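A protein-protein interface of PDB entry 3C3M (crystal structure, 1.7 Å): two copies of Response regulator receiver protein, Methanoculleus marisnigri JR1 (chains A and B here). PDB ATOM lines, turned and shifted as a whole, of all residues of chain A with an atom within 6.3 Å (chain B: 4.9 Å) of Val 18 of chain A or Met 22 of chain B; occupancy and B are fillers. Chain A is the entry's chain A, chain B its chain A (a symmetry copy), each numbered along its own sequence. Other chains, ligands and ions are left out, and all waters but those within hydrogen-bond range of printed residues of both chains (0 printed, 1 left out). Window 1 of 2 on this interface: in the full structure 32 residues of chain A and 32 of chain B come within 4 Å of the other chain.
NH1 of Arg 25 of chain B is in salt-bridge range of OD2 of Asp 17 of chain A. The side-chain hydroxyl of Thr 21 of chain A lies within hydrogen-bond range of the side-chain hydroxyl of Thr 21 of chain B (2.7 Å). OH of Tyr 114 of chain A sits at hydrogen-bond distance from O of Met 22 of chain B. OH of Tyr 114 of chain A is in hydrogen-bond range of N of Gly 26 of chain B (3.1 Å).
OG1 of Thr 21 of chain A lies within hydrogen-bond range of O of Asp 17 of chain A (3.3 Å).
Among the printed residues, pairs that only touch across the chains: Pro 13 of chain A with Arg 25 of chain B, Met 14 of chain A with Met 22 of chain B, Met 14 of chain A with Arg 25 of chain B, Asp 17 of chain A with Thr 21 of chain B, Val 18 of chain A with Met 22 of chain B, Met 22 of chain A with Val 18 of chain B, Thr 109 of chain A with Phe 19 of chain B, Thr 109 of chain A with Met 22 of chain B, His 110 of chain A with Met 22 of chain B, Leu 113 of chain A with Phe 19 of chain B, Leu 113 of chain A with Leu 23 of chain B and Tyr 114 of chain A with Arg 25 of chain B.
Printed residues of chain B within 4 Å of Asp 17 of chain A: Thr 21 and Arg 25. Of chain B, only Met 22 (3.8 Å) comes within 4 Å of Val 18 of chain A. Of the printed residues of chain B, Met 22 of chain A touches Val 18. Leu 23 of chain A touches none of the printed residues of chain B. Printed residues of chain B within 4 Å of Leu 113 of chain A: Phe 19 (3.8 Å) and Leu 23 (3.9 Å). Printed residues of chain B within 4 Å of Tyr 114 of chain A: Met 22, Arg 25 and Gly 26. Val 20 of chain B touches none of the printed residues of chain A. Of chain A, only Met 14 (3.8 Å), Val 18 (3.8 Å), Thr 109 (3.9 Å), His 110 (3.9 Å) and Tyr 114 (2.6 Å) come within 4 Å of Met 22 of chain B. The nearest residue of chain B that does not touch Val 18 of chain A is Val 18 of chain B (4.1 Å). The nearest printed residue of chain A that does not touch Gly 26 of chain B is Met 14 of chain A (5.5 Å).
Hydrophobic or aromatic side chains of chain B within 4 Å of the printed part of chain A: Val 18, Phe 19, Met 22 and Leu 23. Along chain A the printed residues that touch a printed residue of chain B span positions 13 to 114.
Val 18 of chain A touches Met 22 of chain B, and with the chains exchanged Met 22 of chain A touches Val 18 of chain B. Thr 21 of chain A touches its own counterpart, Thr 21 of chain B. 6 positions are printed for both chains. Of the 16 pairs that touch across the chains among the printed residues, 3 have their exchanged pair printed and touching as well.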
ATOM      1  N   PRO A  13     -25.508  26.185  26.908  1.00  0.00           N
ATOM      2  CA  PRO A  13     -24.151  26.595  26.575  1.00  0.00           C
ATOM      3  C   PRO A  13     -23.972  26.796  25.063  1.00  0.00           C
ATOM      4  O   PRO A  13     -23.068  27.538  24.669  1.00  0.00           O
ATOM      5  CB  PRO A  13     -23.294  25.449  27.106  1.00  0.00           C
ATOM      6  CG  PRO A  13     -24.173  24.276  27.142  1.00  0.00           C
ATOM      7  CD  PRO A  13     -25.553  24.796  27.421  1.00  0.00           C
ATOM      8  N   MET A  14     -24.836  26.174  24.250  1.00  0.00           N
ATOM      9  CA  MET A  14     -24.881  26.434  22.788  1.00  0.00           C
ATOM     10  C   MET A  14     -25.306  27.881  22.509  1.00  0.00           C
ATOM     11  O   MET A  14     -24.615  28.616  21.800  1.00  0.00           O
ATOM     12  CB  MET A  14     -25.832  25.467  22.075  1.00  0.00           C
ATOM     13  CG  MET A  14     -26.192  25.858  20.625  1.00  0.00           C
ATOM     14  SD  MET A  14     -24.658  25.598  19.408  1.00  0.00           S
ATOM     15  CE  MET A  14     -24.739  23.661  19.301  1.00  0.00           C
ATOM     16  N   ILE A  15     -26.426  28.286  23.095  1.00  0.00           N
ATOM     17  CA  ILE A  15     -26.908  29.666  22.958  1.00  0.00           C
ATOM     18  C   ILE A  15     -25.856  30.660  23.446  1.00  0.00           C
ATOM     19  O   ILE A  15     -25.559  31.632  22.752  1.00  0.00           O
ATOM     20  CB  ILE A  15     -28.249  29.864  23.724  1.00  0.00           C
ATOM     21  CG1 ILE A  15     -29.368  29.017  23.104  1.00  0.00           C
ATOM     22  CG2 ILE A  15     -28.652  31.348  23.757  1.00  0.00           C
ATOM     23  CD1 ILE A  15     -29.740  29.361  21.687  1.00  0.00           C
ATOM     24  N   VAL A  16     -25.265  30.396  24.613  1.00  0.00           N
ATOM     25  CA  VAL A  16     -24.254  31.304  25.167  1.00  0.00           C
ATOM     26  C   VAL A  16     -23.070  31.427  24.198  1.00  0.00           C
ATOM     27  O   VAL A  16     -22.618  32.528  23.884  1.00  0.00           O
ATOM     28  CB  VAL A  16     -23.776  30.861  26.576  1.00  0.00           C
ATOM     29  CG1 VAL A  16     -22.601  31.698  27.050  1.00  0.00           C
ATOM     30  CG2 VAL A  16     -24.907  30.994  27.601  1.00  0.00           C
ATOM     31  N   ASP A  17     -22.601  30.298  23.690  1.00  0.00           N
ATOM     32  CA  ASP A  17     -21.401  30.316  22.807  1.00  0.00           C
ATOM     33  C   ASP A  17     -21.698  31.056  21.492  1.00  0.00           C
ATOM     34  O   ASP A  17     -20.835  31.764  20.958  1.00  0.00           O
ATOM     35  CB  ASP A  17     -20.982  28.883  22.534  1.00  0.00           C
ATOM     36  CG  ASP A  17     -19.500  28.715  22.353  1.00  0.00           C
ATOM     37  OD1 ASP A  17     -18.731  29.707  22.424  1.00  0.00           O
ATOM     38  OD2 ASP A  17     -19.100  27.553  22.121  1.00  0.00           O
ATOM     39  N   VAL A  18     -22.920  30.910  20.985  1.00  0.00           N
ATOM     40  CA  VAL A  18     -23.316  31.559  19.732  1.00  0.00           C
ATOM     41  C   VAL A  18     -23.350  33.080  19.937  1.00  0.00           C
ATOM     42  O   VAL A  18     -22.772  33.830  19.136  1.00  0.00           O
ATOM     43  CB  VAL A  18     -24.652  31.001  19.218  1.00  0.00           C
ATOM     44  CG1 VAL A  18     -25.258  31.916  18.135  1.00  0.00           C
ATOM     45  CG2 VAL A  18     -24.417  29.602  18.651  1.00  0.00           C
ATOM     46  N   PHE A  19     -23.965  33.529  21.035  1.00  0.00           N
ATOM     47  CA  PHE A  19     -23.925  34.957  21.367  1.00  0.00           C
ATOM     48  C   PHE A  19     -22.509  35.487  21.606  1.00  0.00           C
ATOM     49  O   PHE A  19     -22.181  36.606  21.176  1.00  0.00           O
ATOM     50  CB  PHE A  19     -24.849  35.272  22.543  1.00  0.00           C
ATOM     51  CG  PHE A  19     -26.278  35.426  22.137  1.00  0.00           C
ATOM     52  CD1 PHE A  19     -26.741  36.620  21.607  1.00  0.00           C
ATOM     53  CD2 PHE A  19     -27.157  34.366  22.237  1.00  0.00           C
ATOM     54  CE1 PHE A  19     -28.066  36.761  21.200  1.00  0.00           C
ATOM     55  CE2 PHE A  19     -28.484  34.494  21.821  1.00  0.00           C
ATOM     56  CZ  PHE A  19     -28.939  35.703  21.302  1.00  0.00           C
ATOM     57  N   VAL A  20     -21.660  34.700  22.269  1.00  0.00           N
ATOM     58  CA  VAL A  20     -20.264  35.089  22.460  1.00  0.00           C
ATOM     59  C   VAL A  20     -19.562  35.348  21.109  1.00  0.00           C
ATOM     60  O   VAL A  20     -18.913  36.381  20.925  1.00  0.00           O
ATOM     61  CB  VAL A  20     -19.491  34.049  23.305  1.00  0.00           C
ATOM     62  CG1 VAL A  20     -18.004  34.293  23.256  1.00  0.00           C
ATOM     63  CG2 VAL A  20     -19.953  34.141  24.781  1.00  0.00           C
ATOM     64  N   THR A  21     -19.712  34.415  20.172  1.00  0.00           N
ATOM     65  CA  THR A  21     -19.151  34.611  18.831  1.00  0.00           C
ATOM     66  C   THR A  21     -19.674  35.892  18.170  1.00  0.00           C
ATOM     67  O   THR A  21     -18.878  36.685  17.670  1.00  0.00           O
ATOM     68  CB  THR A  21     -19.430  33.388  17.974  1.00  0.00           C
ATOM     69  OG1 THR A  21     -18.718  32.291  18.548  1.00  0.00           O
ATOM     70  CG2 THR A  21     -18.971  33.600  16.504  1.00  0.00           C
ATOM     71  N   MET A  22     -20.992  36.103  18.203  1.00  0.00           N
ATOM     72  CA  MET A  22     -21.590  37.292  17.588  1.00  0.00           C
ATOM     73  C   MET A  22     -21.049  38.578  18.190  1.00  0.00           C
ATOM     74  O   MET A  22     -20.690  39.501  17.456  1.00  0.00           O
ATOM     75  CB  MET A  22     -23.115  37.256  17.703  1.00  0.00           C
ATOM     76  CG  MET A  22     -23.748  36.148  16.878  1.00  0.00           C
ATOM     77  SD  MET A  22     -25.673  36.150  17.154  1.00  0.00           S
ATOM     78  CE  MET A  22     -26.177  34.781  15.808  1.00  0.00           C
ATOM     79  N   LEU A  23     -20.969  38.619  19.526  1.00  0.00           N
ATOM     80  CA  LEU A  23     -20.507  39.815  20.249  1.00  0.00           C
ATOM     81  C   LEU A  23     -19.031  40.079  20.001  1.00  0.00           C
ATOM     82  O   LEU A  23     -18.644  41.209  19.724  1.00  0.00           O
ATOM     83  CB  LEU A  23     -20.797  39.670  21.743  1.00  0.00           C
ATOM     84  CG  LEU A  23     -22.295  39.693  22.033  1.00  0.00           C
ATOM     85  CD1 LEU A  23     -22.573  39.179  23.457  1.00  0.00           C
ATOM     86  CD2 LEU A  23     -22.896  41.082  21.804  1.00  0.00           C
ATOM     87  N   PRO A 107     -31.830  32.290  18.565  1.00  0.00           N
ATOM     88  CA  PRO A 107     -31.755  31.555  17.312  1.00  0.00           C
ATOM     89  C   PRO A 107     -32.132  30.090  17.549  1.00  0.00           C
ATOM     90  O   PRO A 107     -31.932  29.580  18.659  1.00  0.00           O
ATOM     91  CB  PRO A 107     -30.278  31.665  16.932  1.00  0.00           C
ATOM     92  CG  PRO A 107     -29.566  31.823  18.201  1.00  0.00           C
ATOM     93  CD  PRO A 107     -30.496  32.593  19.116  1.00  0.00           C
ATOM     94  N   THR A 108     -32.694  29.444  16.527  1.00  0.00           N
ATOM     95  CA  THR A 108     -33.048  28.028  16.606  1.00  0.00           C
ATOM     96  C   THR A 108     -32.233  27.176  15.641  1.00  0.00           C
ATOM     97  O   THR A 108     -32.401  25.946  15.606  1.00  0.00           O
ATOM     98  CB  THR A 108     -34.543  27.769  16.320  1.00  0.00           C
ATOM     99  OG1 THR A 108     -34.829  28.087  14.953  1.00  0.00           O
ATOM    100  CG2 THR A 108     -35.442  28.599  17.243  1.00  0.00           C
ATOM    101  N   THR A 109     -31.347  27.832  14.887  1.00  0.00           N
ATOM    102  CA  THR A 109     -30.635  27.247  13.743  1.00  0.00           C
ATOM    103  C   THR A 109     -29.920  25.938  14.044  1.00  0.00           C
ATOM    104  O   THR A 109     -29.948  25.026  13.225  1.00  0.00           O
ATOM    105  CB  THR A 109     -29.606  28.238  13.161  1.00  0.00           C
ATOM    106  OG1 THR A 109     -30.190  29.553  13.103  1.00  0.00           O
ATOM    107  CG2 THR A 109     -29.164  27.810  11.747  1.00  0.00           C
ATOM    108  N   HIS A 110     -29.293  25.860  15.210  1.00  0.00           N
ATOM    109  CA  HIS A 110     -28.544  24.657  15.601  1.00  0.00           C
ATOM    110  C   HIS A 110     -29.401  23.397  15.582  1.00  0.00           C
ATOM    111  O   HIS A 110     -28.933  22.341  15.164  1.00  0.00           O
ATOM    112  CB  HIS A 110     -27.845  24.831  16.959  1.00  0.00           C
ATOM    113  CG  HIS A 110     -28.719  25.399  18.030  1.00  0.00           C
ATOM    114  ND1 HIS A 110     -29.215  26.686  17.983  1.00  0.00           N
ATOM    115  CD2 HIS A 110     -29.168  24.862  19.188  1.00  0.00           C
ATOM    116  CE1 HIS A 110     -29.945  26.910  19.060  1.00  0.00           C
ATOM    117  NE2 HIS A 110     -29.919  25.823  19.812  1.00  0.00           N
ATOM    118  N   LEU A 113     -29.871  22.579  11.927  1.00  0.00           N
ATOM    119  CA  LEU A 113     -28.556  22.241  11.390  1.00  0.00           C
ATOM    120  C   LEU A 113     -28.139  20.805  11.760  1.00  0.00           C
ATOM    121  O   LEU A 113     -27.778  20.014  10.875  1.00  0.00           O
ATOM    122  CB  LEU A 113     -27.512  23.240  11.885  1.00  0.00           C
ATOM    123  CG  LEU A 113     -26.063  22.944  11.514  1.00  0.00           C
ATOM    124  CD1 LEU A 113     -25.815  23.129  10.019  1.00  0.00           C
ATOM    125  CD2 LEU A 113     -25.145  23.822  12.329  1.00  0.00           C
ATOM    126  N   TYR A 114     -28.203  20.465  13.051  1.00  0.00           N
ATOM    127  CA  TYR A 114     -27.744  19.139  13.477  1.00  0.00           C
ATOM    128  C   TYR A 114     -28.655  18.051  12.898  1.00  0.00           C
ATOM    129  O   TYR A 114     -28.173  17.035  12.412  1.00  0.00           O
ATOM    130  CB  TYR A 114     -27.715  19.044  15.011  1.00  0.00           C
ATOM    131  CG  TYR A 114     -26.493  19.632  15.700  1.00  0.00           C
ATOM    132  CD1 TYR A 114     -25.842  20.798  15.224  1.00  0.00           C
ATOM    133  CD2 TYR A 114     -25.997  19.029  16.868  1.00  0.00           C
ATOM    134  CE1 TYR A 114     -24.720  21.327  15.909  1.00  0.00           C
ATOM    135  CE2 TYR A 114     -24.928  19.547  17.548  1.00  0.00           C
ATOM    136  CZ  TYR A 114     -24.276  20.686  17.067  1.00  0.00           C
ATOM    137  OH  TYR A 114     -23.218  21.168  17.765  1.00  0.00           O
ATOM    138  N   VAL B  18     -20.581  31.913  13.000  1.00  0.00           N
ATOM    139  CA  VAL B  18     -21.671  31.399  13.834  1.00  0.00           C
ATOM    140  C   VAL B  18     -21.848  29.898  13.570  1.00  0.00           C
ATOM    141  O   VAL B  18     -21.904  29.100  14.518  1.00  0.00           O
ATOM    142  CB  VAL B  18     -22.964  32.197  13.608  1.00  0.00           C
ATOM    143  CG1 VAL B  18     -24.186  31.449  14.176  1.00  0.00           C
ATOM    144  CG2 VAL B  18     -22.825  33.562  14.280  1.00  0.00           C
ATOM    145  N   PHE B  19     -21.871  29.507  12.292  1.00  0.00           N
ATOM    146  CA  PHE B  19     -21.905  28.079  11.962  1.00  0.00           C
ATOM    147  C   PHE B  19     -20.683  27.308  12.466  1.00  0.00           C
ATOM    148  O   PHE B  19     -20.818  26.171  12.950  1.00  0.00           O
ATOM    149  CB  PHE B  19     -22.125  27.868  10.464  1.00  0.00           C
ATOM    150  CG  PHE B  19     -23.559  27.975  10.064  1.00  0.00           C
ATOM    151  CD1 PHE B  19     -24.423  26.902  10.221  1.00  0.00           C
ATOM    152  CD2 PHE B  19     -24.067  29.161   9.573  1.00  0.00           C
ATOM    153  CE1 PHE B  19     -25.768  27.005   9.875  1.00  0.00           C
ATOM    154  CE2 PHE B  19     -25.417  29.278   9.236  1.00  0.00           C
ATOM    155  CZ  PHE B  19     -26.270  28.188   9.387  1.00  0.00           C
ATOM    156  N   VAL B  20     -19.495  27.909  12.376  1.00  0.00           N
ATOM    157  CA  VAL B  20     -18.290  27.282  12.917  1.00  0.00           C
ATOM    158  C   VAL B  20     -18.444  26.973  14.422  1.00  0.00           C
ATOM    159  O   VAL B  20     -18.169  25.856  14.867  1.00  0.00           O
ATOM    160  CB  VAL B  20     -17.029  28.137  12.644  1.00  0.00           C
ATOM    161  CG1 VAL B  20     -15.848  27.649  13.444  1.00  0.00           C
ATOM    162  CG2 VAL B  20     -16.669  28.054  11.140  1.00  0.00           C
ATOM    163  N   THR B  21     -18.898  27.962  15.189  1.00  0.00           N
ATOM    164  CA  THR B  21     -19.155  27.738  16.617  1.00  0.00           C
ATOM    165  C   THR B  21     -20.151  26.595  16.850  1.00  0.00           C
ATOM    166  O   THR B  21     -19.875  25.704  17.652  1.00  0.00           O
ATOM    167  CB  THR B  21     -19.627  29.029  17.261  1.00  0.00           C
ATOM    168  OG1 THR B  21     -18.548  29.963  17.192  1.00  0.00           O
ATOM    169  CG2 THR B  21     -20.038  28.813  18.745  1.00  0.00           C
ATOM    170  N   MET B  22     -21.274  26.607  16.129  1.00  0.00           N
ATOM    171  CA  MET B  22     -22.294  25.566  16.289  1.00  0.00           C
ATOM    172  C   MET B  22     -21.744  24.180  15.994  1.00  0.00           C
ATOM    173  O   MET B  22     -21.978  23.246  16.762  1.00  0.00           O
ATOM    174  CB  MET B  22     -23.508  25.852  15.403  1.00  0.00           C
ATOM    175  CG  MET B  22     -24.280  27.088  15.832  1.00  0.00           C
ATOM    176  SD  MET B  22     -25.752  27.396  14.599  1.00  0.00           S
ATOM    177  CE  MET B  22     -26.642  28.892  15.553  1.00  0.00           C
ATOM    178  N   LEU B  23     -20.992  24.063  14.892  1.00  0.00           N
ATOM    179  CA  LEU B  23     -20.432  22.774  14.457  1.00  0.00           C
ATOM    180  C   LEU B  23     -19.366  22.278  15.420  1.00  0.00           C
ATOM    181  O   LEU B  23     -19.374  21.113  15.804  1.00  0.00           O
ATOM    182  CB  LEU B  23     -19.877  22.895  13.037  1.00  0.00           C
ATOM    183  CG  LEU B  23     -20.988  23.110  12.014  1.00  0.00           C
ATOM    184  CD1 LEU B  23     -20.397  23.595  10.677  1.00  0.00           C
ATOM    185  CD2 LEU B  23     -21.844  21.854  11.832  1.00  0.00           C
ATOM    186  N   GLU B  24     -18.480  23.179  15.847  1.00  0.00           N
ATOM    187  CA  GLU B  24     -17.395  22.787  16.763  1.00  0.00           C
ATOM    188  C   GLU B  24     -17.899  22.223  18.078  1.00  0.00           C
ATOM    189  O   GLU B  24     -17.346  21.239  18.568  1.00  0.00           O
ATOM    190  CB  GLU B  24     -16.422  23.936  17.012  1.00  0.00           C
ATOM    191  CG  GLU B  24     -15.470  24.115  15.832  1.00  0.00           C
ATOM    192  CD  GLU B  24     -14.449  25.232  15.971  1.00  0.00           C
ATOM    193  OE1 GLU B  24     -14.679  26.175  16.753  1.00  0.00           O
ATOM    194  OE2 GLU B  24     -13.423  25.163  15.249  1.00  0.00           O
ATOM    195  N   ARG B  25     -18.955  22.814  18.638  1.00  0.00           N
ATOM    196  CA  ARG B  25     -19.481  22.319  19.933  1.00  0.00           C
ATOM    197  C   ARG B  25     -19.914  20.847  19.835  1.00  0.00           C
ATOM    198  O   ARG B  25     -19.833  20.100  20.813  1.00  0.00           O
ATOM    199  CB  ARG B  25     -20.657  23.179  20.403  1.00  0.00           C
ATOM    200  CG  ARG B  25     -20.250  24.578  20.824  1.00  0.00           C
ATOM    201  CD  ARG B  25     -21.414  25.246  21.606  1.00  0.00           C
ATOM    202  NE  ARG B  25     -21.711  24.459  22.804  1.00  0.00           N
ATOM    203  CZ  ARG B  25     -20.985  24.503  23.921  1.00  0.00           C
ATOM    204  NH1 ARG B  25     -19.950  25.346  24.042  1.00  0.00           N
ATOM    205  NH2 ARG B  25     -21.300  23.699  24.927  1.00  0.00           N
ATOM    206  N   GLY B  26     -20.326  20.445  18.631  1.00  0.00           N
ATOM    207  CA  GLY B  26     -20.821  19.102  18.378  1.00  0.00           C
ATOM    208  C   GLY B  26     -19.746  18.167  17.861  1.00  0.00           C
ATOM    209  O   GLY B  26     -20.042  17.030  17.509  1.00  0.00           O
